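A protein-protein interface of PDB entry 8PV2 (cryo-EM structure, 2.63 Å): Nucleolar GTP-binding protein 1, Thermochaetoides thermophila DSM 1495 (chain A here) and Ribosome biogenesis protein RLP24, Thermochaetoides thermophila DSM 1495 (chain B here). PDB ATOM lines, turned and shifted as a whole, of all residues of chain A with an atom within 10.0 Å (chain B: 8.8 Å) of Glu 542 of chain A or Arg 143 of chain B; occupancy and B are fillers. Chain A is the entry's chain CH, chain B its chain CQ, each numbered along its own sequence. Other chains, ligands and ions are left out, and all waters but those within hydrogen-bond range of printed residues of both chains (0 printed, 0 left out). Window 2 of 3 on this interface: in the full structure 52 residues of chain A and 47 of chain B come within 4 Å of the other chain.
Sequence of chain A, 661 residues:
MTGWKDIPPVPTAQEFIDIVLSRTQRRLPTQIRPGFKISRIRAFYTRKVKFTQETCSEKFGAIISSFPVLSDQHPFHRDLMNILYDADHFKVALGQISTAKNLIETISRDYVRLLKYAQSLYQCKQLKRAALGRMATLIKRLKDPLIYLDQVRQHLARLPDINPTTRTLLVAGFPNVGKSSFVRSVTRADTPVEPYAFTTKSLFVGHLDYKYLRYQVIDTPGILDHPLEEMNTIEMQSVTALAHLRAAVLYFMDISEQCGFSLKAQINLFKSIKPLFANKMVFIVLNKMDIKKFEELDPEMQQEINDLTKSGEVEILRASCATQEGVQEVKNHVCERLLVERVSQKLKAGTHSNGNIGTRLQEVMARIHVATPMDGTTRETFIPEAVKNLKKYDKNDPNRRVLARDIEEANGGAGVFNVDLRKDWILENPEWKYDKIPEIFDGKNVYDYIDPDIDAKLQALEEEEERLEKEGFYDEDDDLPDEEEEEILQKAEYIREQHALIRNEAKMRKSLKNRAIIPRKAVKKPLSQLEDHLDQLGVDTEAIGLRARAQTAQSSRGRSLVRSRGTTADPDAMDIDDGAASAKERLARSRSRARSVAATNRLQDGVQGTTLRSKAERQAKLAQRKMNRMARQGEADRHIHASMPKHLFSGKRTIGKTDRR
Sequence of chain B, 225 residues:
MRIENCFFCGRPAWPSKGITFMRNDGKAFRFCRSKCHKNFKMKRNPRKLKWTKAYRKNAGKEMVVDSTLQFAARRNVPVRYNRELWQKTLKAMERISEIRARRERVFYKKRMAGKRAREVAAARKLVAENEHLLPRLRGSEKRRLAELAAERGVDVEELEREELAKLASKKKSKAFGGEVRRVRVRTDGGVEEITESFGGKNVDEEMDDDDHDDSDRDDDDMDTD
Among the printed residues, Asp or Glu carboxylates within 4 Å of a Lys or Arg side-chain nitrogen of the other chain: Asp 532 of chain A with Arg 138 of chain B (3.3 Å), Asp 535 of chain A with Arg 138 of chain B (2.6 Å) and Asp 540 of chain A with Arg 143 of chain B (3.4 Å).
The guanidinium group of Arg 143 of chain B is in salt-bridge range of the side-chain carboxylate of Asp 540 of chain A (3.4 Å). The side-chain carboxylate (OD2) of Asp 535 of chain A lies within salt-bridge range of the guanidinium group (NH1) of Arg 138 of chain B (2.6 Å). The backbone carbonyl oxygen of Gly 538 of chain A lies within hydrogen-bond range of the side-chain amino group of Lys 142 of chain B, 3.4 Å away. The backbone NH (N) of Gly 139 of chain B is in hydrogen-bond range of the side-chain carboxylate (OD1) of Asp 535 of chain A. The side-chain carboxylate (OD2) of Asp 535 of chain A sits at hydrogen-bond distance from the side-chain hydroxyl (OG) of Ser 140 of chain B (3.0 Å). The guanidinium group (NH1) of Arg 138 of chain B lies within salt-bridge range of the side-chain carboxylate (OD1) of Asp 532 of chain A, at 3.3 Å.
Among the printed residues, merely in contact across the chains: Val 539 of chain A with Gly 139 of chain B (3.4 Å), Gly 538 of chain A with Leu 137 of chain B (3.7 Å), Glu 542 of chain A with Arg 143 of chain B (3.9 Å) and Gly 538 of chain A with Gly 139 of chain B (3.96 Å).
Of chain B, only Arg 143 comes within 4 Å of Glu 542 of chain A. Arg 143 of chain B touches just these residues of chain A: Asp 540 and Glu 542. No residue of chain B comes within 4 Å of Ala 543 of chain A. Ser 140 of chain B touches just one residue of chain A: Asp 535. Of the printed residues of chain B, Asp 540 of chain A touches Arg 143. Printed residues of chain A within 4 Å of Lys 142 of chain B: Gly 538 (3.4 Å). Leu 534 of chain A touches none of the printed residues of chain B. Ala 150 of chain B touches none of the printed residues of chain A.
The backbone NH (N) of Glu 542 of chain A is in hydrogen-bond range of the side-chain carboxylate (OD2) of Asp 540 of chain A, at 3.1 Å. O of Leu 534 of chain A sits at hydrogen-bond distance from N of Val 539 of chain A (3.2 Å). The backbone NH (N) of Ala 543 of chain A sits at hydrogen-bond distance from the side-chain carboxylate (OD2) of Asp 540 of chain A (2.6 Å).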
ATOM      1  N   LEU A 527      -8.810 -14.218  33.173  1.00  0.00           N
ATOM      2  CA  LEU A 527     -10.078 -14.557  32.535  1.00  0.00           C
ATOM      3  C   LEU A 527     -10.657 -13.376  31.773  1.00  0.00           C
ATOM      4  O   LEU A 527     -11.246 -13.553  30.702  1.00  0.00           O
ATOM      5  CB  LEU A 527     -11.069 -15.052  33.587  1.00  0.00           C
ATOM      6  CG  LEU A 527     -12.441 -15.514  33.103  1.00  0.00           C
ATOM      7  CD1 LEU A 527     -12.315 -16.708  32.182  1.00  0.00           C
ATOM      8  CD2 LEU A 527     -13.312 -15.855  34.295  1.00  0.00           C
ATOM      9  N   GLU A 531     -11.342 -13.584  27.819  1.00  0.00           N
ATOM     10  CA  GLU A 531     -12.699 -13.347  27.339  1.00  0.00           C
ATOM     11  C   GLU A 531     -12.735 -12.184  26.356  1.00  0.00           C
ATOM     12  O   GLU A 531     -13.454 -12.229  25.352  1.00  0.00           O
ATOM     13  CB  GLU A 531     -13.622 -13.086  28.529  1.00  0.00           C
ATOM     14  CG  GLU A 531     -15.083 -13.374  28.269  1.00  0.00           C
ATOM     15  CD  GLU A 531     -15.976 -12.865  29.382  1.00  0.00           C
ATOM     16  OE1 GLU A 531     -15.647 -11.817  29.974  1.00  0.00           O
ATOM     17  OE2 GLU A 531     -17.003 -13.516  29.671  1.00  0.00           O
ATOM     18  N   ASP A 532     -11.945 -11.141  26.622  1.00  0.00           N
ATOM     19  CA  ASP A 532     -11.867 -10.008  25.706  1.00  0.00           C
ATOM     20  C   ASP A 532     -11.265 -10.418  24.367  1.00  0.00           C
ATOM     21  O   ASP A 532     -11.738  -9.991  23.309  1.00  0.00           O
ATOM     22  CB  ASP A 532     -11.053  -8.883  26.342  1.00  0.00           C
ATOM     23  CG  ASP A 532     -11.118  -7.596  25.548  1.00  0.00           C
ATOM     24  OD1 ASP A 532     -12.060  -7.432  24.746  1.00  0.00           O
ATOM     25  OD2 ASP A 532     -10.223  -6.745  25.727  1.00  0.00           O
ATOM     26  N   LEU A 534     -11.259 -13.461  23.021  1.00  0.00           N
ATOM     27  CA  LEU A 534     -12.227 -14.297  22.321  1.00  0.00           C
ATOM     28  C   LEU A 534     -13.376 -13.464  21.765  1.00  0.00           C
ATOM     29  O   LEU A 534     -13.916 -13.769  20.694  1.00  0.00           O
ATOM     30  CB  LEU A 534     -12.744 -15.389  23.255  1.00  0.00           C
ATOM     31  CG  LEU A 534     -11.737 -16.470  23.648  1.00  0.00           C
ATOM     32  CD1 LEU A 534     -12.426 -17.592  24.400  1.00  0.00           C
ATOM     33  CD2 LEU A 534     -11.018 -17.007  22.425  1.00  0.00           C
ATOM     34  N   ASP A 535     -13.751 -12.393  22.468  1.00  0.00           N
ATOM     35  CA  ASP A 535     -14.796 -11.507  21.971  1.00  0.00           C
ATOM     36  C   ASP A 535     -14.317 -10.724  20.754  1.00  0.00           C
ATOM     37  O   ASP A 535     -15.089 -10.471  19.823  1.00  0.00           O
ATOM     38  CB  ASP A 535     -15.248 -10.572  23.090  1.00  0.00           C
ATOM     39  CG  ASP A 535     -16.590  -9.936  22.813  1.00  0.00           C
ATOM     40  OD1 ASP A 535     -17.392 -10.545  22.075  1.00  0.00           O
ATOM     41  OD2 ASP A 535     -16.852  -8.841  23.351  1.00  0.00           O
ATOM     42  N   GLY A 538     -14.593 -13.010  17.948  1.00  0.00           N
ATOM     43  CA  GLY A 538     -15.968 -13.109  17.504  1.00  0.00           C
ATOM     44  C   GLY A 538     -16.672 -14.395  17.859  1.00  0.00           C
ATOM     45  O   GLY A 538     -17.366 -14.965  17.013  1.00  0.00           O
ATOM     46  N   VAL A 539     -16.515 -14.873  19.088  1.00  0.00           N
ATOM     47  CA  VAL A 539     -17.184 -16.076  19.561  1.00  0.00           C
ATOM     48  C   VAL A 539     -18.054 -15.704  20.752  1.00  0.00           C
ATOM     49  O   VAL A 539     -17.881 -14.637  21.352  1.00  0.00           O
ATOM     50  CB  VAL A 539     -16.180 -17.181  19.941  1.00  0.00           C
ATOM     51  CG1 VAL A 539     -15.248 -17.479  18.781  1.00  0.00           C
ATOM     52  CG2 VAL A 539     -15.397 -16.772  21.162  1.00  0.00           C
ATOM     53  N   ASP A 540     -18.997 -16.580  21.085  1.00  0.00           N
ATOM     54  CA  ASP A 540     -19.884 -16.362  22.224  1.00  0.00           C
ATOM     55  C   ASP A 540     -19.257 -17.014  23.449  1.00  0.00           C
ATOM     56  O   ASP A 540     -19.231 -18.239  23.572  1.00  0.00           O
ATOM     57  CB  ASP A 540     -21.270 -16.929  21.939  1.00  0.00           C
ATOM     58  CG  ASP A 540     -22.329 -16.374  22.872  1.00  0.00           C
ATOM     59  OD1 ASP A 540     -23.235 -15.664  22.388  1.00  0.00           O
ATOM     60  OD2 ASP A 540     -22.262 -16.647  24.089  1.00  0.00           O
ATOM     61  N   THR A 541     -18.743 -16.188  24.361  1.00  0.00           N
ATOM     62  CA  THR A 541     -18.122 -16.723  25.568  1.00  0.00           C
ATOM     63  C   THR A 541     -19.171 -17.192  26.570  1.00  0.00           C
ATOM     64  O   THR A 541     -18.915 -18.098  27.372  1.00  0.00           O
ATOM     65  CB  THR A 541     -17.210 -15.673  26.197  1.00  0.00           C
ATOM     66  OG1 THR A 541     -17.997 -14.560  26.637  1.00  0.00           O
ATOM     67  CG2 THR A 541     -16.190 -15.192  25.182  1.00  0.00           C
ATOM     68  N   GLU A 542     -20.356 -16.581  26.544  1.00  0.00           N
ATOM     69  CA  GLU A 542     -21.417 -17.004  27.452  1.00  0.00           C
ATOM     70  C   GLU A 542     -22.001 -18.345  27.032  1.00  0.00           C
ATOM     71  O   GLU A 542     -22.528 -19.090  27.865  1.00  0.00           O
ATOM     72  CB  GLU A 542     -22.507 -15.936  27.519  1.00  0.00           C
ATOM     73  CG  GLU A 542     -22.053 -14.629  28.148  1.00  0.00           C
ATOM     74  CD  GLU A 542     -21.722 -14.771  29.622  1.00  0.00           C
ATOM     75  OE1 GLU A 542     -22.354 -15.607  30.301  1.00  0.00           O
ATOM     76  OE2 GLU A 542     -20.827 -14.044  30.103  1.00  0.00           O
ATOM     77  N   ALA A 543     -21.920 -18.670  25.740  1.00  0.00           N
ATOM     78  CA  ALA A 543     -22.397 -19.964  25.272  1.00  0.00           C
ATOM     79  C   ALA A 543     -21.468 -21.102  25.670  1.00  0.00           C
ATOM     80  O   ALA A 543     -21.902 -22.259  25.695  1.00  0.00           O
ATOM     81  CB  ALA A 543     -22.574 -19.948  23.754  1.00  0.00           C
ATOM     82  N   ILE A 544     -20.204 -20.808  25.979  1.00  0.00           N
ATOM     83  CA  ILE A 544     -19.258 -21.846  26.373  1.00  0.00           C
ATOM     84  C   ILE A 544     -18.963 -21.838  27.866  1.00  0.00           C
ATOM     85  O   ILE A 544     -18.492 -22.859  28.395  1.00  0.00           O
ATOM     86  CB  ILE A 544     -17.943 -21.740  25.570  1.00  0.00           C
ATOM     87  CG1 ILE A 544     -17.203 -20.444  25.900  1.00  0.00           C
ATOM     88  CG2 ILE A 544     -18.227 -21.820  24.080  1.00  0.00           C
ATOM     89  CD1 ILE A 544     -15.901 -20.278  25.155  1.00  0.00           C
ATOM     90  N   GLY A 545     -19.231 -20.737  28.566  1.00  0.00           N
ATOM     91  CA  GLY A 545     -19.098 -20.714  30.009  1.00  0.00           C
ATOM     92  C   GLY A 545     -17.672 -20.788  30.513  1.00  0.00           C
ATOM     93  O   GLY A 545     -17.268 -21.797  31.097  1.00  0.00           O
ATOM     94  N   LEU A 546     -16.896 -19.726  30.292  1.00  0.00           N
ATOM     95  CA  LEU A 546     -15.508 -19.719  30.740  1.00  0.00           C
ATOM     96  C   LEU A 546     -15.395 -19.584  32.254  1.00  0.00           C
ATOM     97  O   LEU A 546     -14.326 -19.855  32.817  1.00  0.00           O
ATOM     98  CB  LEU A 546     -14.741 -18.593  30.052  1.00  0.00           C
ATOM     99  CG  LEU A 546     -14.593 -18.711  28.537  1.00  0.00           C
ATOM    100  CD1 LEU A 546     -14.075 -17.412  27.954  1.00  0.00           C
ATOM    101  CD2 LEU A 546     -13.667 -19.860  28.193  1.00  0.00           C
ATOM    102  N   ARG A 547     -16.472 -19.159  32.922  1.00  0.00           N
ATOM    103  CA  ARG A 547     -16.448 -19.012  34.374  1.00  0.00           C
ATOM    104  C   ARG A 547     -16.243 -20.354  35.064  1.00  0.00           C
ATOM    105  O   ARG A 547     -15.510 -20.448  36.055  1.00  0.00           O
ATOM    106  CB  ARG A 547     -17.747 -18.369  34.858  1.00  0.00           C
ATOM    107  CG  ARG A 547     -17.986 -16.954  34.364  1.00  0.00           C
ATOM    108  CD  ARG A 547     -17.013 -15.962  34.972  1.00  0.00           C
ATOM    109  NE  ARG A 547     -17.329 -14.595  34.577  1.00  0.00           N
ATOM    110  CZ  ARG A 547     -16.831 -13.985  33.510  1.00  0.00           C
ATOM    111  NH1 ARG A 547     -16.005 -14.604  32.684  1.00  0.00           N
ATOM    112  NH2 ARG A 547     -17.178 -12.726  33.260  1.00  0.00           N
ATOM    113  N   ALA A 548     -16.894 -21.404  34.557  1.00  0.00           N
ATOM    114  CA  ALA A 548     -16.724 -22.733  35.133  1.00  0.00           C
ATOM    115  C   ALA A 548     -15.327 -23.278  34.870  1.00  0.00           C
ATOM    116  O   ALA A 548     -14.742 -23.944  35.733  1.00  0.00           O
ATOM    117  CB  ALA A 548     -17.785 -23.683  34.581  1.00  0.00           C
ATOM    118  N   ARG A 549     -14.778 -23.014  33.683  1.00  0.00           N
ATOM    119  CA  ARG A 549     -13.445 -23.504  33.353  1.00  0.00           C
ATOM    120  C   ARG A 549     -12.347 -22.784  34.119  1.00  0.00           C
ATOM    121  O   ARG A 549     -11.316 -23.396  34.419  1.00  0.00           O
ATOM    122  CB  ARG A 549     -13.185 -23.369  31.854  1.00  0.00           C
ATOM    123  CG  ARG A 549     -14.029 -24.273  30.986  1.00  0.00           C
ATOM    124  CD  ARG A 549     -13.649 -24.105  29.530  1.00  0.00           C
ATOM    125  NE  ARG A 549     -14.457 -24.951  28.664  1.00  0.00           N
ATOM    126  CZ  ARG A 549     -15.598 -24.574  28.106  1.00  0.00           C
ATOM    127  NH1 ARG A 549     -16.106 -23.372  28.320  1.00  0.00           N
ATOM    128  NH2 ARG A 549     -16.250 -25.427  27.322  1.00  0.00           N
ATOM    129  N   LEU B 137     -17.527  -8.355  13.913  1.00  0.00           N
ATOM    130  CA  LEU B 137     -18.245  -7.943  15.108  1.00  0.00           C
ATOM    131  C   LEU B 137     -17.870  -8.824  16.291  1.00  0.00           C
ATOM    132  O   LEU B 137     -17.459  -9.976  16.131  1.00  0.00           O
ATOM    133  CB  LEU B 137     -19.756  -8.001  14.888  1.00  0.00           C
ATOM    134  CG  LEU B 137     -20.344  -6.985  13.915  1.00  0.00           C
ATOM    135  CD1 LEU B 137     -21.832  -7.203  13.777  1.00  0.00           C
ATOM    136  CD2 LEU B 137     -20.045  -5.577  14.383  1.00  0.00           C
ATOM    137  N   ARG B 138     -18.024  -8.266  17.488  1.00  0.00           N
ATOM    138  CA  ARG B 138     -17.825  -9.026  18.711  1.00  0.00           C
ATOM    139  C   ARG B 138     -18.913 -10.080  18.871  1.00  0.00           C
ATOM    140  O   ARG B 138     -19.996  -9.977  18.293  1.00  0.00           O
ATOM    141  CB  ARG B 138     -17.841  -8.101  19.923  1.00  0.00           C
ATOM    142  CG  ARG B 138     -16.609  -7.249  20.127  1.00  0.00           C
ATOM    143  CD  ARG B 138     -16.866  -6.314  21.289  1.00  0.00           C
ATOM    144  NE  ARG B 138     -15.703  -5.538  21.696  1.00  0.00           N
ATOM    145  CZ  ARG B 138     -14.868  -5.896  22.661  1.00  0.00           C
ATOM    146  NH1 ARG B 138     -14.990  -7.056  23.284  1.00  0.00           N
ATOM    147  NH2 ARG B 138     -13.898  -5.063  23.022  1.00  0.00           N
ATOM    148  N   GLY B 139     -18.613 -11.107  19.667  1.00  0.00           N
ATOM    149  CA  GLY B 139     -19.634 -12.086  20.004  1.00  0.00           C
ATOM    150  C   GLY B 139     -20.740 -11.502  20.861  1.00  0.00           C
ATOM    151  O   GLY B 139     -21.920 -11.805  20.663  1.00  0.00           O
ATOM    152  N   SER B 140     -20.372 -10.653  21.824  1.00  0.00           N
ATOM    153  CA  SER B 140     -21.370  -9.967  22.638  1.00  0.00           C
ATOM    154  C   SER B 140     -22.215  -9.024  21.793  1.00  0.00           C
ATOM    155  O   SER B 140     -23.433  -8.927  21.985  1.00  0.00           O
ATOM    156  CB  SER B 140     -20.686  -9.201  23.768  1.00  0.00           C
ATOM    157  OG  SER B 140     -19.777  -8.244  23.250  1.00  0.00           O
ATOM    158  N   GLU B 141     -21.584  -8.326  20.847  1.00  0.00           N
ATOM    159  CA  GLU B 141     -22.323  -7.452  19.942  1.00  0.00           C
ATOM    160  C   GLU B 141     -23.254  -8.254  19.043  1.00  0.00           C
ATOM    161  O   GLU B 141     -24.378  -7.827  18.767  1.00  0.00           O
ATOM    162  CB  GLU B 141     -21.354  -6.617  19.108  1.00  0.00           C
ATOM    163  CG  GLU B 141     -20.605  -5.570  19.909  1.00  0.00           C
ATOM    164  CD  GLU B 141     -21.513  -4.468  20.410  1.00  0.00           C
ATOM    165  OE1 GLU B 141     -22.491  -4.140  19.707  1.00  0.00           O
ATOM    166  OE2 GLU B 141     -21.252  -3.933  21.508  1.00  0.00           O
ATOM    167  N   LYS B 142     -22.804  -9.422  18.578  1.00  0.00           N
ATOM    168  CA  LYS B 142     -23.660 -10.282  17.766  1.00  0.00           C
ATOM    169  C   LYS B 142     -24.860 -10.780  18.561  1.00  0.00           C
ATOM    170  O   LYS B 142     -25.982 -10.819  18.044  1.00  0.00           O
ATOM    171  CB  LYS B 142     -22.861 -11.463  17.221  1.00  0.00           C
ATOM    172  CG  LYS B 142     -22.316 -11.257  15.822  1.00  0.00           C
ATOM    173  CD  LYS B 142     -20.969 -11.934  15.654  1.00  0.00           C
ATOM    174  CE  LYS B 142     -21.127 -13.351  15.126  1.00  0.00           C
ATOM    175  NZ  LYS B 142     -19.816 -13.981  14.811  1.00  0.00           N
ATOM    176  N   ARG B 143     -24.641 -11.157  19.823  1.00  0.00           N
ATOM    177  CA  ARG B 143     -25.742 -11.606  20.672  1.00  0.00           C
ATOM    178  C   ARG B 143     -26.728 -10.473  20.942  1.00  0.00           C
ATOM    179  O   ARG B 143     -27.951 -10.680  20.937  1.00  0.00           O
ATOM    180  CB  ARG B 143     -25.186 -12.169  21.980  1.00  0.00           C
ATOM    181  CG  ARG B 143     -26.228 -12.787  22.894  1.00  0.00           C
ATOM    182  CD  ARG B 143     -25.583 -13.382  24.137  1.00  0.00           C
ATOM    183  NE  ARG B 143     -24.957 -12.362  24.971  1.00  0.00           N
ATOM    184  CZ  ARG B 143     -23.651 -12.264  25.182  1.00  0.00           C
ATOM    185  NH1 ARG B 143     -22.796 -13.107  24.628  1.00  0.00           N
ATOM    186  NH2 ARG B 143     -23.193 -11.293  25.968  1.00  0.00           N
ATOM    187  N   ARG B 144     -26.212  -9.262  21.175  1.00  0.00           N
ATOM    188  CA  ARG B 144     -27.086  -8.124  21.440  1.00  0.00           C
ATOM    189  C   ARG B 144     -27.873  -7.741  20.190  1.00  0.00           C
ATOM    190  O   ARG B 144     -29.056  -7.391  20.275  1.00  0.00           O
ATOM    191  CB  ARG B 144     -26.257  -6.953  21.984  1.00  0.00           C
ATOM    192  CG  ARG B 144     -27.040  -5.737  22.500  1.00  0.00           C
ATOM    193  CD  ARG B 144     -27.313  -4.662  21.460  1.00  0.00           C
ATOM    194  NE  ARG B 144     -26.080  -4.095  20.931  1.00  0.00           N
ATOM    195  CZ  ARG B 144     -26.004  -3.376  19.820  1.00  0.00           C
ATOM    196  NH1 ARG B 144     -27.076  -3.113  19.094  1.00  0.00           N
ATOM    197  NH2 ARG B 144     -24.824  -2.898  19.435  1.00  0.00           N
ATOM    198  N   LEU B 145     -27.243  -7.831  19.016  1.00  0.00           N
ATOM    199  CA  LEU B 145     -27.959  -7.593  17.769  1.00  0.00           C
ATOM    200  C   LEU B 145     -29.020  -8.657  17.533  1.00  0.00           C
ATOM    201  O   LEU B 145     -30.107  -8.354  17.034  1.00  0.00           O
ATOM    202  CB  LEU B 145     -26.986  -7.564  16.595  1.00  0.00           C
ATOM    203  CG  LEU B 145     -26.094  -6.337  16.447  1.00  0.00           C
ATOM    204  CD1 LEU B 145     -25.249  -6.490  15.207  1.00  0.00           C
ATOM    205  CD2 LEU B 145     -26.901  -5.063  16.404  1.00  0.00           C
ATOM    206  N   ALA B 146     -28.720  -9.911  17.881  1.00  0.00           N
ATOM    207  CA  ALA B 146     -29.688 -10.987  17.700  1.00  0.00           C
ATOM    208  C   ALA B 146     -30.909 -10.789  18.589  1.00  0.00           C
ATOM    209  O   ALA B 146     -32.051 -10.935  18.137  1.00  0.00           O
ATOM    210  CB  ALA B 146     -29.028 -12.336  17.983  1.00  0.00           C
ATOM    211  N   GLU B 147     -30.690 -10.429  19.858  1.00  0.00           N
ATOM    212  CA  GLU B 147     -31.832 -10.226  20.746  1.00  0.00           C
ATOM    213  C   GLU B 147     -32.600  -8.959  20.376  1.00  0.00           C
ATOM    214  O   GLU B 147     -33.831  -8.919  20.499  1.00  0.00           O
ATOM    215  CB  GLU B 147     -31.387 -10.204  22.213  1.00  0.00           C
ATOM    216  CG  GLU B 147     -30.451  -9.081  22.622  1.00  0.00           C
ATOM    217  CD  GLU B 147     -31.185  -7.854  23.131  1.00  0.00           C
ATOM    218  OE1 GLU B 147     -32.364  -7.988  23.522  1.00  0.00           O
ATOM    219  OE2 GLU B 147     -30.588  -6.758  23.137  1.00  0.00           O
ATOM    220  N   LEU B 148     -31.905  -7.927  19.884  1.00  0.00           N
ATOM    221  CA  LEU B 148     -32.599  -6.721  19.449  1.00  0.00           C
ATOM    222  C   LEU B 148     -33.410  -6.987  18.186  1.00  0.00           C
ATOM    223  O   LEU B 148     -34.503  -6.436  18.014  1.00  0.00           O
ATOM    224  CB  LEU B 148     -31.587  -5.589  19.243  1.00  0.00           C
ATOM    225  CG  LEU B 148     -32.009  -4.140  18.958  1.00  0.00           C
ATOM    226  CD1 LEU B 148     -30.912  -3.212  19.455  1.00  0.00           C
ATOM    227  CD2 LEU B 148     -32.291  -3.854  17.486  1.00  0.00           C
ATOM    228  N   ALA B 149     -32.893  -7.834  17.291  1.00  0.00           N
ATOM    229  CA  ALA B 149     -33.644  -8.216  16.100  1.00  0.00           C
ATOM    230  C   ALA B 149     -34.856  -9.058  16.463  1.00  0.00           C
ATOM    231  O   ALA B 149     -35.917  -8.928  15.843  1.00  0.00           O
ATOM    232  CB  ALA B 149     -32.741  -8.976  15.130  1.00  0.00           C
ATOM    233  N   ALA B 150     -34.718  -9.929  17.466  1.00  0.00           N
ATOM    234  CA  ALA B 150     -35.865 -10.698  17.938  1.00  0.00           C
ATOM    235  C   ALA B 150     -36.913  -9.792  18.575  1.00  0.00           C
ATOM    236  O   ALA B 150     -38.118 -10.037  18.445  1.00  0.00           O
ATOM    237  CB  ALA B 150     -35.410 -11.770  18.926  1.00  0.00           C
ATOM    238  N   VAL B 156     -31.303  -9.440  11.409  1.00  0.00           N
ATOM    239  CA  VAL B 156     -30.046  -9.506  12.146  1.00  0.00           C
ATOM    240  C   VAL B 156     -28.866  -9.243  11.225  1.00  0.00           C
ATOM    241  O   VAL B 156     -27.884  -8.614  11.632  1.00  0.00           O
ATOM    242  CB  VAL B 156     -29.911 -10.863  12.863  1.00  0.00           C
ATOM    243  N   LEU B 159     -28.724  -5.452  10.825  1.00  0.00           N
ATOM    244  CA  LEU B 159     -28.132  -4.847  12.017  1.00  0.00           C
ATOM    245  C   LEU B 159     -26.629  -5.080  12.059  1.00  0.00           C
ATOM    246  O   LEU B 159     -25.860  -4.177  12.418  1.00  0.00           O
ATOM    247  CB  LEU B 159     -28.783  -5.410  13.279  1.00  0.00           C
ATOM    248  CG  LEU B 159     -30.294  -5.300  13.479  1.00  0.00           C
ATOM    249  CD1 LEU B 159     -30.684  -5.929  14.795  1.00  0.00           C
ATOM    250  CD2 LEU B 159     -30.775  -3.873  13.421  1.00  0.00           C
ATOM    251  N   GLU B 160     -26.196  -6.274  11.645  1.00  0.00           N
ATOM    252  CA  GLU B 160     -24.774  -6.573  11.554  1.00  0.00           C
ATOM    253  C   GLU B 160     -24.080  -5.678  10.537  1.00  0.00           C
ATOM    254  O   GLU B 160     -22.945  -5.248  10.761  1.00  0.00           O
ATOM    255  CB  GLU B 160     -24.560  -8.046  11.206  1.00  0.00           C
ATOM    256  CG  GLU B 160     -24.756  -9.005  12.364  1.00  0.00           C
ATOM    257  CD  GLU B 160     -24.752 -10.454  11.920  1.00  0.00           C
ATOM    258  OE1 GLU B 160     -24.811 -10.708  10.697  1.00  0.00           O
ATOM    259  OE2 GLU B 160     -24.693 -11.342  12.795  1.00  0.00           O
